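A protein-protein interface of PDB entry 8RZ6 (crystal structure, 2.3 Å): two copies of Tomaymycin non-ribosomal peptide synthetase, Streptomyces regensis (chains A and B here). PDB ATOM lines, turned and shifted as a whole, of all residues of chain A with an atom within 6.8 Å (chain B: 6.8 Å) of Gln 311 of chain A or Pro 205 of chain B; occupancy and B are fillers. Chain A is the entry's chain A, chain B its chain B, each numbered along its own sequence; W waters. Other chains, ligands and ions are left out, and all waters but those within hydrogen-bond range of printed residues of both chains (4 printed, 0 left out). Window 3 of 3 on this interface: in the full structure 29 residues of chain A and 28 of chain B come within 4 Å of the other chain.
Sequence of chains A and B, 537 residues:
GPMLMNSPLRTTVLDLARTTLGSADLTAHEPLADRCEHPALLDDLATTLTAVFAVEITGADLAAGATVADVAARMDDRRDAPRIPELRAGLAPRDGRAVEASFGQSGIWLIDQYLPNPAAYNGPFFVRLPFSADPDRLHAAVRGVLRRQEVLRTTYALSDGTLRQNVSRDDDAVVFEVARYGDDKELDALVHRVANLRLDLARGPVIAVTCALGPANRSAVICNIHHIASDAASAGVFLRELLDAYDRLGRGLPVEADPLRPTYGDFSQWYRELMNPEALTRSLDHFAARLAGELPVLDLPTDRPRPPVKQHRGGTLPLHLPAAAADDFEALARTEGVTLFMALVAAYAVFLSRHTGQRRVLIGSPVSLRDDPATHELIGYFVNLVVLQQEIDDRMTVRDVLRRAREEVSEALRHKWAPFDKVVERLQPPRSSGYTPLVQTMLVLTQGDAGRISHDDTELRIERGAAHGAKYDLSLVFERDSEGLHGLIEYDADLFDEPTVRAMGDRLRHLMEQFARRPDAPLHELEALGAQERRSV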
ATOM      1  N   PRO A 116       9.571  15.898  12.867  1.00  0.00           N
ATOM      2  CA  PRO A 116       9.723  16.115  11.424  1.00  0.00           C
ATOM      3  C   PRO A 116       8.601  17.005  10.894  1.00  0.00           C
ATOM      4  O   PRO A 116       7.614  17.325  11.582  1.00  0.00           O
ATOM      5  CB  PRO A 116       9.691  14.698  10.833  1.00  0.00           C
ATOM      6  CG  PRO A 116       9.102  13.835  11.896  1.00  0.00           C
ATOM      7  CD  PRO A 116       9.364  14.480  13.218  1.00  0.00           C
ATOM      8  N   PRO A 307      -0.303   3.313  18.421  1.00  0.00           N
ATOM      9  CA  PRO A 307       0.626   2.986  19.488  1.00  0.00           C
ATOM     10  C   PRO A 307       0.633   4.063  20.556  1.00  0.00           C
ATOM     11  O   PRO A 307       0.329   5.235  20.284  1.00  0.00           O
ATOM     12  CB  PRO A 307       1.983   2.911  18.766  1.00  0.00           C
ATOM     13  CG  PRO A 307       1.842   3.895  17.649  1.00  0.00           C
ATOM     14  CD  PRO A 307       0.394   3.823  17.225  1.00  0.00           C
ATOM     15  N   VAL A 309       3.273   5.402  21.871  1.00  0.00           N
ATOM     16  CA  VAL A 309       4.333   6.302  21.451  1.00  0.00           C
ATOM     17  C   VAL A 309       4.184   6.483  19.946  1.00  0.00           C
ATOM     18  O   VAL A 309       4.293   5.516  19.179  1.00  0.00           O
ATOM     19  CB  VAL A 309       5.720   5.729  21.800  1.00  0.00           C
ATOM     20  CG1 VAL A 309       6.803   6.631  21.279  1.00  0.00           C
ATOM     21  CG2 VAL A 309       5.869   5.568  23.296  1.00  0.00           C
ATOM     22  N   LYS A 310       3.887   7.702  19.522  1.00  0.00           N
ATOM     23  CA  LYS A 310       3.893   7.995  18.102  1.00  0.00           C
ATOM     24  C   LYS A 310       5.339   8.039  17.617  1.00  0.00           C
ATOM     25  O   LYS A 310       6.193   8.658  18.256  1.00  0.00           O
ATOM     26  CB  LYS A 310       3.179   9.313  17.823  1.00  0.00           C
ATOM     27  CG  LYS A 310       3.018   9.623  16.334  1.00  0.00           C
ATOM     28  CD  LYS A 310       2.400  11.020  16.115  1.00  0.00           C
ATOM     29  CE  LYS A 310       1.510  11.066  14.909  1.00  0.00           C
ATOM     30  NZ  LYS A 310       2.099  10.504  13.708  1.00  0.00           N
ATOM     31  N   GLN A 311       5.609   7.399  16.484  1.00  0.00           N
ATOM     32  CA  GLN A 311       6.950   7.398  15.907  1.00  0.00           C
ATOM     33  C   GLN A 311       7.141   8.390  14.761  1.00  0.00           C
ATOM     34  O   GLN A 311       8.273   8.506  14.242  1.00  0.00           O
ATOM     35  CB  GLN A 311       7.314   5.980  15.428  1.00  0.00           C
ATOM     36  CG  GLN A 311       7.307   4.931  16.537  1.00  0.00           C
ATOM     37  CD  GLN A 311       8.430   5.145  17.573  1.00  0.00           C
ATOM     38  OE1 GLN A 311       9.409   5.861  17.323  1.00  0.00           O
ATOM     39  NE2 GLN A 311       8.284   4.524  18.730  1.00  0.00           N
ATOM     40  N   HIS A 312       6.070   9.088  14.333  1.00  0.00           N
ATOM     41  CA  HIS A 312       6.167  10.191  13.360  1.00  0.00           C
ATOM     42  C   HIS A 312       6.761   9.702  12.040  1.00  0.00           C
ATOM     43  O   HIS A 312       7.676  10.319  11.479  1.00  0.00           O
ATOM     44  CB  HIS A 312       6.974  11.362  13.950  1.00  0.00           C
ATOM     45  CG  HIS A 312       6.487  11.787  15.308  1.00  0.00           C
ATOM     46  ND1 HIS A 312       5.398  12.623  15.484  1.00  0.00           N
ATOM     47  CD2 HIS A 312       6.913  11.469  16.553  1.00  0.00           C
ATOM     48  CE1 HIS A 312       5.187  12.808  16.775  1.00  0.00           C
ATOM     49  NE2 HIS A 312       6.078  12.106  17.445  1.00  0.00           N
ATOM     50  N   ARG A 313       6.230   8.574  11.542  1.00  0.00           N
ATOM     51  CA  ARG A 313       6.787   7.896  10.370  1.00  0.00           C
ATOM     52  C   ARG A 313       5.742   7.896   9.269  1.00  0.00           C
ATOM     53  O   ARG A 313       4.844   7.030   9.248  1.00  0.00           O
ATOM     54  CB  ARG A 313       7.244   6.466  10.719  1.00  0.00           C
ATOM     55  CG  ARG A 313       6.220   5.607  11.502  1.00  0.00           C
ATOM     56  CD  ARG A 313       6.644   4.153  11.452  1.00  0.00           C
ATOM     57  NE  ARG A 313       5.931   3.290  12.373  1.00  0.00           N
ATOM     58  CZ  ARG A 313       5.810   1.974  12.220  1.00  0.00           C
ATOM     59  NH1 ARG A 313       6.356   1.347  11.187  1.00  0.00           N
ATOM     60  NH2 ARG A 313       5.115   1.274  13.113  1.00  0.00           N
ATOM     61  N   GLY A 314       5.848   8.863   8.369  1.00  0.00           N
ATOM     62  CA  GLY A 314       4.927   8.986   7.275  1.00  0.00           C
ATOM     63  C   GLY A 314       5.390   8.229   6.042  1.00  0.00           C
ATOM     64  O   GLY A 314       6.577   8.196   5.717  1.00  0.00           O
ATOM     65  N   GLY A 469       6.002  13.530   9.061  1.00  0.00           N
ATOM     66  CA  GLY A 469       5.675  13.061  10.388  1.00  0.00           C
ATOM     67  C   GLY A 469       4.306  12.448  10.556  1.00  0.00           C
ATOM     68  O   GLY A 469       3.947  12.058  11.674  1.00  0.00           O
ATOM     69  N   ASP A 492      -0.004   7.449   7.734  1.00  0.00           N
ATOM     70  CA  ASP A 492       0.703   7.157   8.968  1.00  0.00           C
ATOM     71  C   ASP A 492       1.163   5.697   8.959  1.00  0.00           C
ATOM     72  O   ASP A 492       0.336   4.771   9.020  1.00  0.00           O
ATOM     73  CB  ASP A 492      -0.183   7.436  10.173  1.00  0.00           C
ATOM     74  CG  ASP A 492       0.578   7.360  11.473  1.00  0.00           C
ATOM     75  OD1 ASP A 492       1.769   6.914  11.444  1.00  0.00           O
ATOM     76  OD2 ASP A 492      -0.018   7.735  12.517  1.00  0.00           O
ATOM     77  N   ASP A 494       2.580   4.220  11.341  1.00  0.00           N
ATOM     78  CA  ASP A 494       2.252   3.589  12.620  1.00  0.00           C
ATOM     79  C   ASP A 494       0.984   2.737  12.527  1.00  0.00           C
ATOM     80  O   ASP A 494       0.795   1.806  13.332  1.00  0.00           O
ATOM     81  CB  ASP A 494       2.054   4.626  13.730  1.00  0.00           C
ATOM     82  CG  ASP A 494       3.359   5.052  14.387  1.00  0.00           C
ATOM     83  OD1 ASP A 494       4.385   4.356  14.212  1.00  0.00           O
ATOM     84  OD2 ASP A 494       3.354   6.081  15.092  1.00  0.00           O
ATOM     85  N   LEU B 152      16.723  -6.103  23.713  1.00  0.00           N
ATOM     86  CA  LEU B 152      15.640  -5.597  22.861  1.00  0.00           C
ATOM     87  C   LEU B 152      14.329  -5.422  23.607  1.00  0.00           C
ATOM     88  O   LEU B 152      13.390  -4.839  23.053  1.00  0.00           O
ATOM     89  CB  LEU B 152      15.390  -6.525  21.674  1.00  0.00           C
ATOM     90  CG  LEU B 152      16.636  -6.705  20.796  1.00  0.00           C
ATOM     91  CD1 LEU B 152      16.356  -7.622  19.623  1.00  0.00           C
ATOM     92  CD2 LEU B 152      17.149  -5.345  20.309  1.00  0.00           C
ATOM     93  N   THR B 154      14.338  -4.065  26.818  1.00  0.00           N
ATOM     94  CA  THR B 154      14.808  -3.274  27.952  1.00  0.00           C
ATOM     95  C   THR B 154      14.514  -1.796  27.729  1.00  0.00           C
ATOM     96  O   THR B 154      14.693  -1.286  26.623  1.00  0.00           O
ATOM     97  CB  THR B 154      16.331  -3.488  28.173  1.00  0.00           C
ATOM     98  OG1 THR B 154      16.575  -4.859  28.514  1.00  0.00           O
ATOM     99  CG2 THR B 154      16.887  -2.609  29.284  1.00  0.00           C
ATOM    100  N   THR B 155      14.026  -1.136  28.769  1.00  0.00           N
ATOM    101  CA  THR B 155      13.858   0.300  28.852  1.00  0.00           C
ATOM    102  C   THR B 155      14.622   0.778  30.082  1.00  0.00           C
ATOM    103  O   THR B 155      15.047  -0.016  30.919  1.00  0.00           O
ATOM    104  CB  THR B 155      12.379   0.720  28.933  1.00  0.00           C
ATOM    105  OG1 THR B 155      11.738   0.076  30.043  1.00  0.00           O
ATOM    106  CG2 THR B 155      11.639   0.334  27.625  1.00  0.00           C
ATOM    107  N   ASP B 172       6.681  -8.180  21.579  1.00  0.00           N
ATOM    108  CA  ASP B 172       6.161  -7.445  20.432  1.00  0.00           C
ATOM    109  C   ASP B 172       6.528  -5.958  20.477  1.00  0.00           C
ATOM    110  O   ASP B 172       5.962  -5.164  19.721  1.00  0.00           O
ATOM    111  CB  ASP B 172       4.629  -7.603  20.337  1.00  0.00           C
ATOM    112  CG  ASP B 172       4.074  -7.276  18.917  1.00  0.00           C
ATOM    113  OD1 ASP B 172       4.862  -7.350  17.932  1.00  0.00           O
ATOM    114  OD2 ASP B 172       2.855  -6.920  18.773  1.00  0.00           O
ATOM    115  N   ALA B 173       7.463  -5.556  21.342  1.00  0.00           N
ATOM    116  CA  ALA B 173       7.903  -4.159  21.423  1.00  0.00           C
ATOM    117  C   ALA B 173       8.870  -3.846  20.275  1.00  0.00           C
ATOM    118  O   ALA B 173      10.085  -3.718  20.439  1.00  0.00           O
ATOM    119  CB  ALA B 173       8.553  -3.885  22.769  1.00  0.00           C
ATOM    120  N   VAL B 174       8.300  -3.730  19.084  1.00  0.00           N
ATOM    121  CA  VAL B 174       9.071  -3.404  17.890  1.00  0.00           C
ATOM    122  C   VAL B 174       8.250  -2.503  16.976  1.00  0.00           C
ATOM    123  O   VAL B 174       7.039  -2.698  16.797  1.00  0.00           O
ATOM    124  CB  VAL B 174       9.517  -4.685  17.170  1.00  0.00           C
ATOM    125  CG1 VAL B 174       8.322  -5.596  16.929  1.00  0.00           C
ATOM    126  CG2 VAL B 174      10.276  -4.353  15.884  1.00  0.00           C
ATOM    127  N   VAL B 175       8.917  -1.480  16.441  1.00  0.00           N
ATOM    128  CA  VAL B 175       8.330  -0.579  15.443  1.00  0.00           C
ATOM    129  C   VAL B 175       8.385  -1.318  14.111  1.00  0.00           C
ATOM    130  O   VAL B 175       9.459  -1.409  13.501  1.00  0.00           O
ATOM    131  CB  VAL B 175       9.058   0.766  15.372  1.00  0.00           C
ATOM    132  CG1 VAL B 175       8.394   1.658  14.223  1.00  0.00           C
ATOM    133  CG2 VAL B 175       9.045   1.456  16.733  1.00  0.00           C
ATOM    134  N   ASN B 196      15.596   7.202  10.367  1.00  0.00           N
ATOM    135  CA  ASN B 196      15.343   8.495  10.974  1.00  0.00           C
ATOM    136  C   ASN B 196      14.366   8.407  12.154  1.00  0.00           C
ATOM    137  O   ASN B 196      13.988   9.444  12.704  1.00  0.00           O
ATOM    138  CB  ASN B 196      14.846   9.476   9.896  1.00  0.00           C
ATOM    139  CG  ASN B 196      15.868   9.686   8.743  1.00  0.00           C
ATOM    140  OD1 ASN B 196      15.479   9.799   7.582  1.00  0.00           O
ATOM    141  ND2 ASN B 196      17.164   9.736   9.071  1.00  0.00           N
ATOM    142  N   LEU B 197      13.998   7.201  12.595  1.00  0.00           N
ATOM    143  CA  LEU B 197      13.168   7.074  13.792  1.00  0.00           C
ATOM    144  C   LEU B 197      13.952   7.591  15.001  1.00  0.00           C
ATOM    145  O   LEU B 197      15.179   7.531  15.033  1.00  0.00           O
ATOM    146  CB  LEU B 197      12.766   5.621  14.019  1.00  0.00           C
ATOM    147  CG  LEU B 197      11.933   5.004  12.918  1.00  0.00           C
ATOM    148  CD1 LEU B 197      11.781   3.531  13.156  1.00  0.00           C
ATOM    149  CD2 LEU B 197      10.581   5.636  12.929  1.00  0.00           C
ATOM    150  N   ARG B 198      13.250   8.130  15.986  1.00  0.00           N
ATOM    151  CA  ARG B 198      13.871   8.682  17.192  1.00  0.00           C
ATOM    152  C   ARG B 198      13.202   7.914  18.331  1.00  0.00           C
ATOM    153  O   ARG B 198      12.134   8.292  18.824  1.00  0.00           O
ATOM    154  CB  ARG B 198      13.695  10.202  17.314  1.00  0.00           C
ATOM    155  CG  ARG B 198      14.134  11.004  16.067  1.00  0.00           C
ATOM    156  CD  ARG B 198      15.661  11.052  15.847  1.00  0.00           C
ATOM    157  NE  ARG B 198      16.018  11.639  14.552  1.00  0.00           N
ATOM    158  CZ  ARG B 198      16.323  12.919  14.349  1.00  0.00           C
ATOM    159  NH1 ARG B 198      16.347  13.808  15.342  1.00  0.00           N
ATOM    160  NH2 ARG B 198      16.620  13.320  13.118  1.00  0.00           N
ATOM    161  N   LEU B 199      13.822   6.803  18.724  1.00  0.00           N
ATOM    162  CA  LEU B 199      13.183   5.850  19.620  1.00  0.00           C
ATOM    163  C   LEU B 199      13.249   6.331  21.064  1.00  0.00           C
ATOM    164  O   LEU B 199      14.208   6.989  21.462  1.00  0.00           O
ATOM    165  CB  LEU B 199      13.857   4.497  19.454  1.00  0.00           C
ATOM    166  CG  LEU B 199      13.736   3.919  18.037  1.00  0.00           C
ATOM    167  CD1 LEU B 199      14.658   2.721  17.868  1.00  0.00           C
ATOM    168  CD2 LEU B 199      12.289   3.531  17.710  1.00  0.00           C
ATOM    169  N   ASP B 200      12.180   6.057  21.817  1.00  0.00           N
ATOM    170  CA  ASP B 200      12.037   6.481  23.207  1.00  0.00           C
ATOM    171  C   ASP B 200      12.745   5.473  24.125  1.00  0.00           C
ATOM    172  O   ASP B 200      12.438   4.277  24.093  1.00  0.00           O
ATOM    173  CB  ASP B 200      10.542   6.571  23.525  1.00  0.00           C
ATOM    174  CG  ASP B 200      10.248   7.324  24.801  1.00  0.00           C
ATOM    175  OD1 ASP B 200      10.697   6.865  25.877  1.00  0.00           O
ATOM    176  OD2 ASP B 200       9.515   8.340  24.747  1.00  0.00           O
ATOM    177  N   LEU B 201      13.707   5.955  24.920  1.00  0.00           N
ATOM    178  CA  LEU B 201      14.452   5.058  25.795  1.00  0.00           C
ATOM    179  C   LEU B 201      13.702   4.708  27.073  1.00  0.00           C
ATOM    180  O   LEU B 201      13.976   3.662  27.678  1.00  0.00           O
ATOM    181  CB  LEU B 201      15.791   5.681  26.173  1.00  0.00           C
ATOM    182  CG  LEU B 201      16.808   5.787  25.042  1.00  0.00           C
ATOM    183  CD1 LEU B 201      18.137   6.256  25.631  1.00  0.00           C
ATOM    184  CD2 LEU B 201      16.957   4.471  24.277  1.00  0.00           C
ATOM    185  N   ARG B 203      10.202   4.467  27.254  1.00  0.00           N
ATOM    186  CA  ARG B 203       9.026   3.668  26.948  1.00  0.00           C
ATOM    187  C   ARG B 203       9.265   2.593  25.902  1.00  0.00           C
ATOM    188  O   ARG B 203       8.497   1.622  25.851  1.00  0.00           O
ATOM    189  CB  ARG B 203       7.882   4.571  26.454  1.00  0.00           C
ATOM    190  CG  ARG B 203       7.325   5.475  27.520  1.00  0.00           C
ATOM    191  CD  ARG B 203       6.212   6.364  26.982  1.00  0.00           C
ATOM    192  NE  ARG B 203       6.700   7.703  26.676  1.00  0.00           N
ATOM    193  CZ  ARG B 203       6.008   8.623  26.020  1.00  0.00           C
ATOM    194  NH1 ARG B 203       4.787   8.379  25.564  1.00  0.00           N
ATOM    195  NH2 ARG B 203       6.554   9.817  25.814  1.00  0.00           N
ATOM    196  N   GLY B 204      10.278   2.756  25.047  1.00  0.00           N
ATOM    197  CA  GLY B 204      10.482   1.859  23.929  1.00  0.00           C
ATOM    198  C   GLY B 204       9.424   2.082  22.868  1.00  0.00           C
ATOM    199  O   GLY B 204       8.580   2.964  23.003  1.00  0.00           O
ATOM    200  N   PRO B 205       9.458   1.300  21.783  1.00  0.00           N
ATOM    201  CA  PRO B 205      10.463   0.267  21.476  1.00  0.00           C
ATOM    202  C   PRO B 205      11.874   0.801  21.235  1.00  0.00           C
ATOM    203  O   PRO B 205      12.071   1.961  20.860  1.00  0.00           O
ATOM    204  CB  PRO B 205       9.921  -0.394  20.208  1.00  0.00           C
ATOM    205  CG  PRO B 205       8.440  -0.108  20.238  1.00  0.00           C
ATOM    206  CD  PRO B 205       8.305   1.230  20.879  1.00  0.00           C
ATOM    207  N   VAL B 206      12.879  -0.045  21.466  1.00  0.00           N
ATOM    208  CA  VAL B 206      14.269   0.277  21.142  1.00  0.00           C
ATOM    209  C   VAL B 206      14.694  -0.373  19.829  1.00  0.00           C
ATOM    210  O   VAL B 206      15.854  -0.240  19.421  1.00  0.00           O
ATOM    211  CB  VAL B 206      15.224  -0.117  22.286  1.00  0.00           C
ATOM    212  CG1 VAL B 206      14.795   0.608  23.555  1.00  0.00           C
ATOM    213  CG2 VAL B 206      15.194  -1.620  22.534  1.00  0.00           C
ATOM    214  N   ILE B 207      13.760  -1.014  19.117  1.00  0.00           N
ATOM    215  CA  ILE B 207      14.066  -1.624  17.829  1.00  0.00           C
ATOM    216  C   ILE B 207      12.939  -1.340  16.834  1.00  0.00           C
ATOM    217  O   ILE B 207      11.762  -1.327  17.191  1.00  0.00           O
ATOM    218  CB  ILE B 207      14.333  -3.138  17.967  1.00  0.00           C
ATOM    219  CG1 ILE B 207      14.521  -3.776  16.586  1.00  0.00           C
ATOM    220  CG2 ILE B 207      13.211  -3.780  18.743  1.00  0.00           C
ATOM    221  CD1 ILE B 207      15.081  -5.251  16.645  1.00  0.00           C
ATOM    222  N   ALA B 208      13.318  -1.093  15.587  1.00  0.00           N
ATOM    223  CA  ALA B 208      12.414  -1.002  14.458  1.00  0.00           C
ATOM    224  C   ALA B 208      12.849  -2.005  13.404  1.00  0.00           C
ATOM    225  O   ALA B 208      14.051  -2.224  13.181  1.00  0.00           O
ATOM    226  CB  ALA B 208      12.408   0.421  13.864  1.00  0.00           C
ATOM    227  N   HIS B 226      18.390   0.993  18.748  1.00  0.00           N
ATOM    228  CA  HIS B 226      18.992   2.127  19.432  1.00  0.00           C
ATOM    229  C   HIS B 226      20.431   1.824  19.851  1.00  0.00           C
ATOM    230  O   HIS B 226      20.753   0.704  20.282  1.00  0.00           O
ATOM    231  CB  HIS B 226      18.161   2.513  20.662  1.00  0.00           C
ATOM    232  CG  HIS B 226      18.421   3.907  21.141  1.00  0.00           C
ATOM    233  ND1 HIS B 226      19.549   4.246  21.861  1.00  0.00           N
ATOM    234  CD2 HIS B 226      17.727   5.062  20.963  1.00  0.00           C
ATOM    235  CE1 HIS B 226      19.525   5.537  22.133  1.00  0.00           C
ATOM    236  NE2 HIS B 226      18.432   6.055  21.601  1.00  0.00           N
HETATM  237  O   HOH W   1       4.709  -1.481  15.124  1.00  0.00           O
HETATM  238  O   HOH W   2      10.391   7.937  15.973  1.00  0.00           O
HETATM  239  O   HOH W   3       9.929   7.459  19.805  1.00  0.00           O
HETATM  240  O   HOH W   4      10.251   4.061  20.800  1.00  0.00           O
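No position is printed for both chains. Of the 8 pairs that touch across the chains among the printed residues, none has its exchanged pair printed and touching as well.
Arg 203 of chain B touches Val 309 of chain A (NH1 to CG2, 3.8 Å). CG2 of Val 309 of chain A touches O of Gly 204 of chain B, 3.8 Å away. Gln 311 of chain A touches Val 175 of chain B. Leu 197 of chain B touches Gln 311 of chain A (CD2 to O, 3.9 Å). Arg 198 of chain B touches Gln 311 of chain A. CD2 of Leu 199 of chain B touches OE1 of Gln 311 of chain A (3.7 Å). NE2 of Gln 311 of chain A touches CD of Pro 205 of chain B (3.9 Å). Val 175 of chain B touches Arg 313 of chain A.
The side-chain carboxylate (OD2) of Asp 200 of chain B lies within salt-bridge range of the guanidinium group (NE) of Arg 203 of chain B, 3.5 Å away. N of Val 175 of chain B is in hydrogen-bond range of O of Ile 207 of chain B. The side-chain carboxylate (OD1) of Asp 494 of chain A is in salt-bridge range of the guanidinium group (NE) of Arg 313 of chain A (2.6 Å). The backbone NH (N) of Gln 311 of chain A lies within hydrogen-bond range of the side-chain carboxylate (OD2) of Asp 494 of chain A (3.0 Å).
Of the 11 printed residues of chain A, 3 touch a printed residue of chain B. Hydrophobic or aromatic side chains of chain A within 4 Å of the printed part of chain B: Val 309. Of the 20 printed residues of chain B, 7 touch a printed residue of chain A. Among the printed residues, 8 pairs touch across the chains. Among the printed residues, no Asp or Glu carboxylate lies within 4 Å of a Lys or Arg side-chain nitrogen of the other chain.
Water W3 lies within hydrogen-bond range of the backbone carbonyl oxygen (O) of Arg 198 of chain B (2.6 Å), the side-chain amide oxygen (OE1) of Gln 311 of chain A (3.0 Å) and the backbone NH (N) of Asp 200 of chain B (3.3 Å). Water W2 bridges OE1 of Gln 311 of chain A (2.7 Å) and N of Arg 198 of chain B (2.9 Å). Water W4 lies within hydrogen-bond range of the backbone carbonyl oxygen of Pro 205 of chain B, the side-chain amide nitrogen of Gln 311 of chain A, the backbone NH of Asp 200 of chain B and the backbone carbonyl oxygen of Gly 204 of chain B. Water W1 lies within hydrogen-bond range of the backbone carbonyl oxygen (O) of Val 174 of chain B and the guanidinium group (NH2) of Arg 313 of chain A.
Gln 311 of chain A touches just these residues of chain B: Val 175, Leu 197, Arg 198, Leu 199 and Pro 205. Pro 205 of chain B touches one residue of chain A. Of the printed residues of chain A, Arg 203 of chain B touches Val 309. Of the printed residues of chain B, Arg 313 of chain A touches Val 175. Of the printed residues of chain A, Leu 197 of chain B touches Gln 311 (3.9 Å). Printed residues of chain B within 4 Å of Val 309 of chain A: Arg 203 (3.8 Å) and Gly 204 (3.8 Å). Asp 494 of chain A touches none of the printed residues of chain B. The nearest printed residue of chain A that does not touch Leu 199 of chain B is Val 309 of chain A (6.5 Å).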
